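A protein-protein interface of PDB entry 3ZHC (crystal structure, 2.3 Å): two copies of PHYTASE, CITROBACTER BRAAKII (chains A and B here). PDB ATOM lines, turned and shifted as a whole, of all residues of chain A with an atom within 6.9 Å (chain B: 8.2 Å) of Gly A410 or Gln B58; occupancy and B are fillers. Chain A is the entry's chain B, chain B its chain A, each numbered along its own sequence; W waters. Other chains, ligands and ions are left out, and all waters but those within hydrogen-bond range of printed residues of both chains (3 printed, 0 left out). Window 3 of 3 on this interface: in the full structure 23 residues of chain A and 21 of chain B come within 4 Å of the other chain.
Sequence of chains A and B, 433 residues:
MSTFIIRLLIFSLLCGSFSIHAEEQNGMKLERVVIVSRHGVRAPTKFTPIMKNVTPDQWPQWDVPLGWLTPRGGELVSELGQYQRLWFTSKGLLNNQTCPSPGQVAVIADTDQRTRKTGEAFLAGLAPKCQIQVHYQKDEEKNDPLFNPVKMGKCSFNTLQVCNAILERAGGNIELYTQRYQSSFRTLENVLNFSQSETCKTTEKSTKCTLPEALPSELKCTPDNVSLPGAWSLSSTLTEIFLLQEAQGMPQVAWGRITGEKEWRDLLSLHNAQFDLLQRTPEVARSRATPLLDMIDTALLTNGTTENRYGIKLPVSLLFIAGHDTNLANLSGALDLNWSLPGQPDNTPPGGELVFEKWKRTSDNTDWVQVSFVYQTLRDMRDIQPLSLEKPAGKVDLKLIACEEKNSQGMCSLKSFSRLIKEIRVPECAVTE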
ATOM      1  N   TRP A 368     -26.820   2.325 -14.268  1.00  0.00           N
ATOM      2  CA  TRP A 368     -25.816   1.767 -13.360  1.00  0.00           C
ATOM      3  C   TRP A 368     -26.015   2.299 -11.939  1.00  0.00           C
ATOM      4  O   TRP A 368     -26.500   3.416 -11.758  1.00  0.00           O
ATOM      5  CB  TRP A 368     -24.409   2.097 -13.873  1.00  0.00           C
ATOM      6  CG  TRP A 368     -24.236   1.708 -15.330  1.00  0.00           C
ATOM      7  CD1 TRP A 368     -24.554   2.470 -16.427  1.00  0.00           C
ATOM      8  CD2 TRP A 368     -23.733   0.468 -15.840  1.00  0.00           C
ATOM      9  NE1 TRP A 368     -24.272   1.787 -17.583  1.00  0.00           N
ATOM     10  CE2 TRP A 368     -23.766   0.556 -17.260  1.00  0.00           C
ATOM     11  CE3 TRP A 368     -23.245  -0.705 -15.243  1.00  0.00           C
ATOM     12  CZ2 TRP A 368     -23.330  -0.493 -18.090  1.00  0.00           C
ATOM     13  CZ3 TRP A 368     -22.812  -1.753 -16.071  1.00  0.00           C
ATOM     14  CH2 TRP A 368     -22.858  -1.637 -17.479  1.00  0.00           C
ATOM     15  N   VAL A 369     -25.635   1.484 -10.943  1.00  0.00           N
ATOM     16  CA  VAL A 369     -25.798   1.815  -9.525  1.00  0.00           C
ATOM     17  C   VAL A 369     -24.455   1.923  -8.826  1.00  0.00           C
ATOM     18  O   VAL A 369     -23.683   0.966  -8.848  1.00  0.00           O
ATOM     19  CB  VAL A 369     -26.651   0.745  -8.772  1.00  0.00           C
ATOM     20  CG1 VAL A 369     -26.815   1.125  -7.293  1.00  0.00           C
ATOM     21  CG2 VAL A 369     -27.994   0.574  -9.419  1.00  0.00           C
ATOM     22  N   GLN A 370     -24.180   3.089  -8.212  1.00  0.00           N
ATOM     23  CA  GLN A 370     -22.971   3.297  -7.398  1.00  0.00           C
ATOM     24  C   GLN A 370     -23.372   3.399  -5.937  1.00  0.00           C
ATOM     25  O   GLN A 370     -24.372   4.056  -5.614  1.00  0.00           O
ATOM     26  CB  GLN A 370     -22.207   4.562  -7.807  1.00  0.00           C
ATOM     27  CG  GLN A 370     -20.768   4.564  -7.250  1.00  0.00           C
ATOM     28  CD  GLN A 370     -19.958   5.710  -7.736  1.00  0.00           C
ATOM     29  OE1 GLN A 370     -20.352   6.867  -7.586  1.00  0.00           O
ATOM     30  NE2 GLN A 370     -18.793   5.413  -8.326  1.00  0.00           N
ATOM     31  N   ASP A 397     -15.938   4.987  -1.207  1.00  0.00           N
ATOM     32  CA  ASP A 397     -16.508   4.259  -2.333  1.00  0.00           C
ATOM     33  C   ASP A 397     -16.689   2.800  -1.918  1.00  0.00           C
ATOM     34  O   ASP A 397     -15.710   2.124  -1.602  1.00  0.00           O
ATOM     35  CB  ASP A 397     -15.593   4.377  -3.571  1.00  0.00           C
ATOM     36  CG  ASP A 397     -16.295   3.985  -4.887  1.00  0.00           C
ATOM     37  OD1 ASP A 397     -17.423   3.347  -4.869  1.00  0.00           O
ATOM     38  OD2 ASP A 397     -15.711   4.323  -5.960  1.00  0.00           O
ATOM     39  N   LEU A 398     -17.940   2.330  -1.909  1.00  0.00           N
ATOM     40  CA  LEU A 398     -18.257   0.947  -1.541  1.00  0.00           C
ATOM     41  C   LEU A 398     -18.313   0.073  -2.805  1.00  0.00           C
ATOM     42  O   LEU A 398     -18.701   0.555  -3.899  1.00  0.00           O
ATOM     43  CB  LEU A 398     -19.564   0.868  -0.753  1.00  0.00           C
ATOM     44  CG  LEU A 398     -19.618   1.746   0.512  1.00  0.00           C
ATOM     45  CD1 LEU A 398     -20.924   1.557   1.185  1.00  0.00           C
ATOM     46  CD2 LEU A 398     -18.468   1.441   1.493  1.00  0.00           C
ATOM     47  N   LYS A 399     -17.931  -1.204  -2.635  1.00  0.00           N
ATOM     48  CA  LYS A 399     -17.857  -2.167  -3.732  1.00  0.00           C
ATOM     49  C   LYS A 399     -18.857  -3.323  -3.535  1.00  0.00           C
ATOM     50  O   LYS A 399     -18.755  -4.089  -2.553  1.00  0.00           O
ATOM     51  CB  LYS A 399     -16.434  -2.723  -3.849  1.00  0.00           C
ATOM     52  CG  LYS A 399     -15.301  -1.655  -3.884  1.00  0.00           C
ATOM     53  CD  LYS A 399     -15.452  -0.651  -5.020  1.00  0.00           C
ATOM     54  CE  LYS A 399     -14.326   0.402  -4.980  1.00  0.00           C
ATOM     55  NZ  LYS A 399     -14.447   1.429  -6.068  1.00  0.00           N
ATOM     56  N   LEU A 400     -19.820  -3.440  -4.464  1.00  0.00           N
ATOM     57  CA  LEU A 400     -20.784  -4.537  -4.490  1.00  0.00           C
ATOM     58  C   LEU A 400     -20.160  -5.570  -5.421  1.00  0.00           C
ATOM     59  O   LEU A 400     -20.465  -5.608  -6.615  1.00  0.00           O
ATOM     60  CB  LEU A 400     -22.172  -4.090  -4.987  1.00  0.00           C
ATOM     61  CG  LEU A 400     -23.158  -3.548  -3.979  1.00  0.00           C
ATOM     62  CD1 LEU A 400     -24.371  -2.978  -4.692  1.00  0.00           C
ATOM     63  CD2 LEU A 400     -23.569  -4.650  -3.014  1.00  0.00           C
ATOM     64  N   ILE A 401     -19.287  -6.404  -4.853  1.00  0.00           N
ATOM     65  CA  ILE A 401     -18.501  -7.411  -5.610  1.00  0.00           C
ATOM     66  C   ILE A 401     -19.365  -8.527  -6.260  1.00  0.00           C
ATOM     67  O   ILE A 401     -19.061  -8.981  -7.374  1.00  0.00           O
ATOM     68  CB  ILE A 401     -17.415  -8.059  -4.708  1.00  0.00           C
ATOM     69  CG1 ILE A 401     -16.405  -7.010  -4.219  1.00  0.00           C
ATOM     70  CG2 ILE A 401     -16.667  -9.161  -5.449  1.00  0.00           C
ATOM     71  CD1 ILE A 401     -15.475  -7.540  -3.171  1.00  0.00           C
ATOM     72  N   ALA A 402     -20.427  -8.948  -5.563  1.00  0.00           N
ATOM     73  CA  ALA A 402     -21.332 -10.028  -6.038  1.00  0.00           C
ATOM     74  C   ALA A 402     -22.079  -9.747  -7.365  1.00  0.00           C
ATOM     75  O   ALA A 402     -22.593 -10.693  -7.984  1.00  0.00           O
ATOM     76  CB  ALA A 402     -22.349 -10.379  -4.943  1.00  0.00           C
ATOM     77  N   CYS A 403     -22.150  -8.466  -7.790  1.00  0.00           N
ATOM     78  CA  CYS A 403     -22.807  -8.084  -9.064  1.00  0.00           C
ATOM     79  C   CYS A 403     -22.194  -8.785 -10.262  1.00  0.00           C
ATOM     80  O   CYS A 403     -20.974  -8.928 -10.343  1.00  0.00           O
ATOM     81  CB  CYS A 403     -22.744  -6.563  -9.297  1.00  0.00           C
ATOM     82  SG  CYS A 403     -23.883  -5.608  -8.324  1.00  0.00           S
ATOM     83  N   GLU A 405     -22.707  -7.911 -13.752  1.00  0.00           N
ATOM     84  CA  GLU A 405     -22.290  -6.928 -14.741  1.00  0.00           C
ATOM     85  C   GLU A 405     -21.764  -5.675 -14.037  1.00  0.00           C
ATOM     86  O   GLU A 405     -22.495  -5.057 -13.246  1.00  0.00           O
ATOM     87  CB  GLU A 405     -23.480  -6.550 -15.640  1.00  0.00           C
ATOM     88  CG  GLU A 405     -24.294  -7.750 -16.239  1.00  0.00           C
ATOM     89  CD  GLU A 405     -25.793  -7.405 -16.465  1.00  0.00           C
ATOM     90  OE1 GLU A 405     -26.100  -6.415 -17.181  1.00  0.00           O
ATOM     91  OE2 GLU A 405     -26.658  -8.129 -15.900  1.00  0.00           O
ATOM     92  N   LYS A 406     -20.503  -5.308 -14.325  1.00  0.00           N
ATOM     93  CA  LYS A 406     -19.856  -4.103 -13.772  1.00  0.00           C
ATOM     94  C   LYS A 406     -19.370  -3.125 -14.866  1.00  0.00           C
ATOM     95  O   LYS A 406     -19.070  -3.535 -15.985  1.00  0.00           O
ATOM     96  CB  LYS A 406     -18.624  -4.468 -12.895  1.00  0.00           C
ATOM     97  CG  LYS A 406     -18.845  -4.611 -11.369  1.00  0.00           C
ATOM     98  CD  LYS A 406     -19.370  -5.973 -10.942  1.00  0.00           C
ATOM     99  CE  LYS A 406     -19.004  -6.268  -9.461  1.00  0.00           C
ATOM    100  NZ  LYS A 406     -17.511  -6.592  -9.261  1.00  0.00           N
ATOM    101  N   ASN A 407     -19.299  -1.837 -14.495  1.00  0.00           N
ATOM    102  CA  ASN A 407     -18.701  -0.759 -15.327  1.00  0.00           C
ATOM    103  C   ASN A 407     -17.199  -0.785 -15.308  1.00  0.00           C
ATOM    104  O   ASN A 407     -16.587  -1.526 -14.537  1.00  0.00           O
ATOM    105  CB  ASN A 407     -19.144   0.664 -14.815  1.00  0.00           C
ATOM    106  CG  ASN A 407     -20.349   1.195 -15.487  1.00  0.00           C
ATOM    107  OD1 ASN A 407     -20.968   2.126 -14.986  1.00  0.00           O
ATOM    108  ND2 ASN A 407     -20.699   0.636 -16.629  1.00  0.00           N
ATOM    109  N   SER A 408     -16.597   0.042 -16.173  1.00  0.00           N
ATOM    110  CA  SER A 408     -15.147   0.296 -16.144  1.00  0.00           C
ATOM    111  C   SER A 408     -14.814   1.090 -14.872  1.00  0.00           C
ATOM    112  O   SER A 408     -13.724   0.936 -14.307  1.00  0.00           O
ATOM    113  CB  SER A 408     -14.690   1.061 -17.386  1.00  0.00           C
ATOM    114  OG  SER A 408     -15.361   2.318 -17.498  1.00  0.00           O
ATOM    115  N   GLN A 409     -15.770   1.940 -14.439  1.00  0.00           N
ATOM    116  CA  GLN A 409     -15.682   2.712 -13.196  1.00  0.00           C
ATOM    117  C   GLN A 409     -16.317   1.981 -11.934  1.00  0.00           C
ATOM    118  O   GLN A 409     -16.679   2.636 -10.954  1.00  0.00           O
ATOM    119  CB  GLN A 409     -16.314   4.102 -13.416  1.00  0.00           C
ATOM    120  CG  GLN A 409     -15.743   5.226 -12.513  1.00  0.00           C
ATOM    121  CD  GLN A 409     -16.221   6.630 -12.927  1.00  0.00           C
ATOM    122  OE1 GLN A 409     -17.151   6.781 -13.750  1.00  0.00           O
ATOM    123  NE2 GLN A 409     -15.585   7.669 -12.353  1.00  0.00           N
ATOM    124  N   GLY A 410     -16.444   0.644 -11.982  1.00  0.00           N
ATOM    125  CA  GLY A 410     -16.891  -0.171 -10.811  1.00  0.00           C
ATOM    126  C   GLY A 410     -18.373  -0.237 -10.422  1.00  0.00           C
ATOM    127  O   GLY A 410     -18.733  -0.942  -9.464  1.00  0.00           O
ATOM    128  N   MET A 411     -19.228   0.481 -11.142  1.00  0.00           N
ATOM    129  CA  MET A 411     -20.672   0.503 -10.843  1.00  0.00           C
ATOM    130  C   MET A 411     -21.382  -0.765 -11.298  1.00  0.00           C
ATOM    131  O   MET A 411     -21.073  -1.304 -12.354  1.00  0.00           O
ATOM    132  CB  MET A 411     -21.359   1.683 -11.524  1.00  0.00           C
ATOM    133  CG  MET A 411     -20.761   3.044 -11.241  1.00  0.00           C
ATOM    134  SD  MET A 411     -21.788   4.302 -11.970  1.00  0.00           S
ATOM    135  CE  MET A 411     -20.714   5.733 -11.886  1.00  0.00           C
ATOM    136  N   CYS A 412     -22.335  -1.220 -10.486  1.00  0.00           N
ATOM    137  CA  CYS A 412     -23.139  -2.379 -10.803  1.00  0.00           C
ATOM    138  C   CYS A 412     -24.174  -1.970 -11.847  1.00  0.00           C
ATOM    139  O   CYS A 412     -24.600  -0.827 -11.863  1.00  0.00           O
ATOM    140  CB  CYS A 412     -23.809  -2.884  -9.526  1.00  0.00           C
ATOM    141  SG  CYS A 412     -24.722  -4.362  -9.688  1.00  0.00           S
ATOM    142  N   PHE B  47      -4.452   2.021  -1.475  1.00  0.00           N
ATOM    143  CA  PHE B  47      -5.409   1.643  -2.494  1.00  0.00           C
ATOM    144  C   PHE B  47      -5.393   2.750  -3.566  1.00  0.00           C
ATOM    145  O   PHE B  47      -5.909   3.842  -3.331  1.00  0.00           O
ATOM    146  CB  PHE B  47      -6.791   1.450  -1.891  1.00  0.00           C
ATOM    147  CG  PHE B  47      -7.820   0.989  -2.881  1.00  0.00           C
ATOM    148  CD1 PHE B  47      -7.647  -0.229  -3.572  1.00  0.00           C
ATOM    149  CD2 PHE B  47      -8.965   1.752  -3.134  1.00  0.00           C
ATOM    150  CE1 PHE B  47      -8.593  -0.679  -4.501  1.00  0.00           C
ATOM    151  CE2 PHE B  47      -9.927   1.308  -4.067  1.00  0.00           C
ATOM    152  CZ  PHE B  47      -9.738   0.092  -4.750  1.00  0.00           C
ATOM    153  N   MET B  51      -3.983   0.021  -9.135  1.00  0.00           N
ATOM    154  CA  MET B  51      -4.456  -1.247  -8.549  1.00  0.00           C
ATOM    155  C   MET B  51      -5.824  -1.661  -9.100  1.00  0.00           C
ATOM    156  O   MET B  51      -6.064  -2.845  -9.306  1.00  0.00           O
ATOM    157  CB  MET B  51      -4.511  -1.167  -7.018  1.00  0.00           C
ATOM    158  CG  MET B  51      -3.155  -1.082  -6.358  1.00  0.00           C
ATOM    159  SD  MET B  51      -3.266  -0.739  -4.592  1.00  0.00           S
ATOM    160  CE  MET B  51      -4.209  -2.137  -4.033  1.00  0.00           C
ATOM    161  N   LYS B  52      -6.704  -0.684  -9.333  1.00  0.00           N
ATOM    162  CA  LYS B  52      -8.029  -0.949  -9.934  1.00  0.00           C
ATOM    163  C   LYS B  52      -7.934  -1.256 -11.431  1.00  0.00           C
ATOM    164  O   LYS B  52      -8.660  -2.103 -11.935  1.00  0.00           O
ATOM    165  CB  LYS B  52      -8.952   0.245  -9.791  1.00  0.00           C
ATOM    166  CG  LYS B  52      -9.253   0.692  -8.401  1.00  0.00           C
ATOM    167  CD  LYS B  52     -10.154   1.924  -8.493  1.00  0.00           C
ATOM    168  CE  LYS B  52     -10.539   2.474  -7.164  1.00  0.00           C
ATOM    169  NZ  LYS B  52     -11.442   3.665  -7.358  1.00  0.00           N
ATOM    170  N   THR B  55      -6.756  -4.990 -13.188  1.00  0.00           N
ATOM    171  CA  THR B  55      -7.680  -6.119 -13.131  1.00  0.00           C
ATOM    172  C   THR B  55      -9.126  -5.660 -13.485  1.00  0.00           C
ATOM    173  O   THR B  55      -9.521  -4.573 -13.114  1.00  0.00           O
ATOM    174  CB  THR B  55      -7.662  -6.777 -11.752  1.00  0.00           C
ATOM    175  OG1 THR B  55      -8.589  -7.872 -11.727  1.00  0.00           O
ATOM    176  CG2 THR B  55      -8.012  -5.753 -10.642  1.00  0.00           C
ATOM    177  N   PRO B  56      -9.896  -6.491 -14.221  1.00  0.00           N
ATOM    178  CA  PRO B  56     -11.317  -6.169 -14.460  1.00  0.00           C
ATOM    179  C   PRO B  56     -12.210  -6.422 -13.234  1.00  0.00           C
ATOM    180  O   PRO B  56     -13.323  -5.951 -13.195  1.00  0.00           O
ATOM    181  CB  PRO B  56     -11.698  -7.124 -15.595  1.00  0.00           C
ATOM    182  CG  PRO B  56     -10.845  -8.286 -15.371  1.00  0.00           C
ATOM    183  CD  PRO B  56      -9.518  -7.721 -14.937  1.00  0.00           C
ATOM    184  N   ASP B  57     -11.706  -7.175 -12.259  1.00  0.00           N
ATOM    185  CA  ASP B  57     -12.435  -7.470 -11.025  1.00  0.00           C
ATOM    186  C   ASP B  57     -12.213  -6.371  -9.985  1.00  0.00           C
ATOM    187  O   ASP B  57     -11.307  -5.534 -10.120  1.00  0.00           O
ATOM    188  CB  ASP B  57     -11.988  -8.799 -10.471  1.00  0.00           C
ATOM    189  CG  ASP B  57     -12.254  -9.924 -11.416  1.00  0.00           C
ATOM    190  OD1 ASP B  57     -13.454 -10.248 -11.637  1.00  0.00           O
ATOM    191  OD2 ASP B  57     -11.263 -10.505 -11.953  1.00  0.00           O
ATOM    192  N   GLN B  58     -13.046  -6.384  -8.954  1.00  0.00           N
ATOM    193  CA  GLN B  58     -12.939  -5.432  -7.851  1.00  0.00           C
ATOM    194  C   GLN B  58     -12.223  -6.068  -6.660  1.00  0.00           C
ATOM    195  O   GLN B  58     -12.426  -7.246  -6.357  1.00  0.00           O
ATOM    196  CB  GLN B  58     -14.321  -4.910  -7.450  1.00  0.00           C
ATOM    197  CG  GLN B  58     -14.921  -3.955  -8.492  1.00  0.00           C
ATOM    198  CD  GLN B  58     -16.218  -3.295  -8.022  1.00  0.00           C
ATOM    199  OE1 GLN B  58     -17.105  -3.957  -7.471  1.00  0.00           O
ATOM    200  NE2 GLN B  58     -16.336  -1.977  -8.252  1.00  0.00           N
ATOM    201  N   TRP B  59     -11.383  -5.278  -5.994  1.00  0.00           N
ATOM    202  CA  TRP B  59     -10.659  -5.731  -4.802  1.00  0.00           C
ATOM    203  C   TRP B  59     -11.585  -5.782  -3.587  1.00  0.00           C
ATOM    204  O   TRP B  59     -12.386  -4.880  -3.395  1.00  0.00           O
ATOM    205  CB  TRP B  59      -9.483  -4.795  -4.482  1.00  0.00           C
ATOM    206  CG  TRP B  59      -8.428  -4.813  -5.484  1.00  0.00           C
ATOM    207  CD1 TRP B  59      -8.374  -4.082  -6.622  1.00  0.00           C
ATOM    208  CD2 TRP B  59      -7.265  -5.602  -5.455  1.00  0.00           C
ATOM    209  NE1 TRP B  59      -7.240  -4.363  -7.310  1.00  0.00           N
ATOM    210  CE2 TRP B  59      -6.531  -5.300  -6.620  1.00  0.00           C
ATOM    211  CE3 TRP B  59      -6.753  -6.550  -4.550  1.00  0.00           C
ATOM    212  CZ2 TRP B  59      -5.311  -5.905  -6.915  1.00  0.00           C
ATOM    213  CZ3 TRP B  59      -5.544  -7.152  -4.835  1.00  0.00           C
ATOM    214  CH2 TRP B  59      -4.827  -6.826  -6.017  1.00  0.00           C
ATOM    215  N   PRO B  60     -11.483  -6.841  -2.762  1.00  0.00           N
ATOM    216  CA  PRO B  60     -12.285  -6.849  -1.542  1.00  0.00           C
ATOM    217  C   PRO B  60     -11.827  -5.773  -0.548  1.00  0.00           C
ATOM    218  O   PRO B  60     -10.625  -5.554  -0.401  1.00  0.00           O
ATOM    219  CB  PRO B  60     -12.049  -8.244  -0.981  1.00  0.00           C
ATOM    220  CG  PRO B  60     -10.814  -8.726  -1.624  1.00  0.00           C
ATOM    221  CD  PRO B  60     -10.725  -8.093  -2.930  1.00  0.00           C
ATOM    222  N   GLN B  61     -12.791  -5.118   0.110  1.00  0.00           N
ATOM    223  CA  GLN B  61     -12.505  -4.078   1.088  1.00  0.00           C
ATOM    224  C   GLN B  61     -12.294  -4.671   2.471  1.00  0.00           C
ATOM    225  O   GLN B  61     -12.838  -5.736   2.811  1.00  0.00           O
ATOM    226  CB  GLN B  61     -13.635  -3.059   1.161  1.00  0.00           C
ATOM    227  CG  GLN B  61     -13.890  -2.316  -0.137  1.00  0.00           C
ATOM    228  CD  GLN B  61     -14.948  -1.223   0.023  1.00  0.00           C
ATOM    229  OE1 GLN B  61     -16.069  -1.341  -0.513  1.00  0.00           O
ATOM    230  NE2 GLN B  61     -14.607  -0.156   0.781  1.00  0.00           N
ATOM    231  N   LEU B 192      -4.678 -11.739 -11.924  1.00  0.00           N
ATOM    232  CA  LEU B 192      -5.345 -10.448 -12.150  1.00  0.00           C
ATOM    233  C   LEU B 192      -6.336 -10.428 -13.324  1.00  0.00           C
ATOM    234  O   LEU B 192      -7.131  -9.484 -13.432  1.00  0.00           O
ATOM    235  CB  LEU B 192      -4.298  -9.356 -12.422  1.00  0.00           C
ATOM    236  CG  LEU B 192      -3.332  -8.958 -11.320  1.00  0.00           C
ATOM    237  CD1 LEU B 192      -2.263  -8.045 -11.899  1.00  0.00           C
ATOM    238  CD2 LEU B 192      -4.085  -8.291 -10.171  1.00  0.00           C
ATOM    239  N   GLN B 245      -4.716 -11.183   2.594  1.00  0.00           N
ATOM    240  CA  GLN B 245      -6.115 -11.667   2.409  1.00  0.00           C
ATOM    241  C   GLN B 245      -6.289 -13.106   2.894  1.00  0.00           C
ATOM    242  O   GLN B 245      -7.253 -13.417   3.608  1.00  0.00           O
ATOM    243  CB  GLN B 245      -6.541 -11.621   0.951  1.00  0.00           C
ATOM    244  CG  GLN B 245      -6.773 -10.260   0.349  1.00  0.00           C
ATOM    245  CD  GLN B 245      -7.013 -10.342  -1.173  1.00  0.00           C
ATOM    246  OE1 GLN B 245      -6.921 -11.418  -1.767  1.00  0.00           O
ATOM    247  NE2 GLN B 245      -7.326  -9.198  -1.797  1.00  0.00           N
ATOM    248  N   GLN B 252     -12.927 -14.718  -0.347  1.00  0.00           N
ATOM    249  CA  GLN B 252     -12.467 -14.612  -1.735  1.00  0.00           C
ATOM    250  C   GLN B 252     -11.051 -14.018  -1.791  1.00  0.00           C
ATOM    251  O   GLN B 252     -10.891 -12.790  -1.791  1.00  0.00           O
ATOM    252  CB  GLN B 252     -13.449 -13.750  -2.560  1.00  0.00           C
ATOM    253  CG  GLN B 252     -14.863 -14.299  -2.619  1.00  0.00           C
ATOM    254  CD  GLN B 252     -15.841 -13.339  -3.261  1.00  0.00           C
ATOM    255  OE1 GLN B 252     -15.672 -12.928  -4.411  1.00  0.00           O
ATOM    256  NE2 GLN B 252     -16.880 -12.982  -2.521  1.00  0.00           N
ATOM    257  N   ALA B 254      -7.725 -13.354  -3.853  1.00  0.00           N
ATOM    258  CA  ALA B 254      -7.260 -13.189  -5.252  1.00  0.00           C
ATOM    259  C   ALA B 254      -8.272 -13.749  -6.277  1.00  0.00           C
ATOM    260  O   ALA B 254      -7.899 -14.417  -7.270  1.00  0.00           O
ATOM    261  CB  ALA B 254      -5.892 -13.817  -5.430  1.00  0.00           C
ATOM    262  N   TRP B 255      -9.560 -13.474  -6.010  1.00  0.00           N
ATOM    263  CA  TRP B 255     -10.685 -13.930  -6.848  1.00  0.00           C
ATOM    264  C   TRP B 255     -10.701 -15.457  -7.042  1.00  0.00           C
ATOM    265  O   TRP B 255     -11.241 -15.970  -8.029  1.00  0.00           O
ATOM    266  CB  TRP B 255     -10.664 -13.167  -8.189  1.00  0.00           C
ATOM    267  CG  TRP B 255     -10.526 -11.693  -7.944  1.00  0.00           C
ATOM    268  CD1 TRP B 255     -11.507 -10.847  -7.588  1.00  0.00           C
ATOM    269  CD2 TRP B 255      -9.320 -10.906  -8.024  1.00  0.00           C
ATOM    270  NE1 TRP B 255     -11.012  -9.571  -7.438  1.00  0.00           N
ATOM    271  CE2 TRP B 255      -9.671  -9.578  -7.700  1.00  0.00           C
ATOM    272  CE3 TRP B 255      -7.975 -11.197  -8.342  1.00  0.00           C
ATOM    273  CZ2 TRP B 255      -8.727  -8.523  -7.678  1.00  0.00           C
ATOM    274  CZ3 TRP B 255      -7.029 -10.146  -8.320  1.00  0.00           C
ATOM    275  CH2 TRP B 255      -7.417  -8.827  -7.993  1.00  0.00           C
ATOM    276  N   ARG B 257      -8.166 -17.310  -7.804  1.00  0.00           N
ATOM    277  CA  ARG B 257      -7.242 -17.744  -8.919  1.00  0.00           C
ATOM    278  C   ARG B 257      -5.782 -18.127  -8.534  1.00  0.00           C
ATOM    279  O   ARG B 257      -4.939 -18.304  -9.438  1.00  0.00           O
ATOM    280  CB  ARG B 257      -7.200 -16.675  -9.996  1.00  0.00           C
ATOM    281  CG  ARG B 257      -8.530 -16.377 -10.591  1.00  0.00           C
ATOM    282  CD  ARG B 257      -8.381 -15.507 -11.795  1.00  0.00           C
ATOM    283  NE  ARG B 257      -9.636 -14.866 -12.083  1.00  0.00           N
ATOM    284  CZ  ARG B 257      -9.966 -13.591 -11.845  1.00  0.00           C
ATOM    285  NH1 ARG B 257      -9.116 -12.708 -11.302  1.00  0.00           N
ATOM    286  NH2 ARG B 257     -11.195 -13.191 -12.181  1.00  0.00           N
HETATM  287  O   HOH W   1     -14.959  -8.753  -8.438  1.00  0.00           O
HETATM  288  O   HOH W   2     -19.479  -2.196  -7.210  1.00  0.00           O
HETATM  289  O   HOH W   3     -17.354  -3.619   0.100  1.00  0.00           O
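The side-chain amino group of Lys A406 sits at hydrogen-bond distance from the side-chain amide oxygen of Gln B58, 3.2 Å away.
The backbone carbonyl oxygen (O) of Gly A410 is in hydrogen-bond range of the side-chain amide nitrogen (NE2) of Gln B58 (2.9 Å).
NE2 of Gln B61 sits at hydrogen-bond distance from O of Asp A397 (3.5 Å).
The backbone NH (N) of Lys A399 is in hydrogen-bond range of the side-chain amide oxygen (OE1) of Gln B61 (2.8 Å).
O of Gln B58 is in hydrogen-bond range of NE1 of Trp B255.
The side-chain amino group of Lys A399 lies within salt-bridge range of the side-chain carboxylate of Asp A397.
The backbone carbonyl oxygen of Ile A401 sits at hydrogen-bond distance from the side-chain amino group of Lys A406, at 3.4 Å.
SG of Cys A412 is disulfide-bonded to SG of Cys A403 (2.0 Å).
Among the printed residues, pairs that only touch across the chains: Leu A398 with Gln B61, Lys A399 with Gln B58, Ile A401 with Pro B60, Leu A400 with Gln B58 and Lys A399 with Lys B52.
Of chain B, only Gln B58 comes within 4 Å of Gly A410.
Of the printed residues of chain A, Gln B58 touches Lys A399 (3.6 Å), Leu A400 (3.8 Å), Lys A406 (3.2 Å) and Gly A410 (2.9 Å).
Of the printed residues of chain B, Lys A399 touches Lys B52 (3.96 Å), Gln B58 (3.6 Å) and Gln B61 (2.8 Å).
Printed residues of chain A within 4 Å of Pro B60: Ile A401.
Trp B255 touches none of the printed residues of chain A.
The nearest residue of chain B that does not touch Gly A410 is Pro B56 (7.2 Å).
The nearest printed residue of chain A that does not touch Pro B60 is Lys A399 (6.3 Å).
Among the printed residues, 9 pairs touch across the chains.
Among the printed residues, no Asp or Glu carboxylate lies within 4 Å of a Lys or Arg side-chain nitrogen of the other chain.
No position is printed for both chains.
Of the 9 pairs that touch across the chains among the printed residues, none has its exchanged pair printed and touching as well.
Water W2 lies within hydrogen-bond range of the backbone carbonyl oxygen of Gly A410 (2.7 Å), the side-chain amide oxygen of Gln B58 (3.0 Å) and the backbone NH of Leu A400 (3.0 Å).
Water W3 lies within hydrogen-bond range of OE1 of Gln B61 and O of Lys A399.
Water W1 bridges N of Gln B58 (3.1 Å) and NZ of Lys A406 (3.4 Å).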
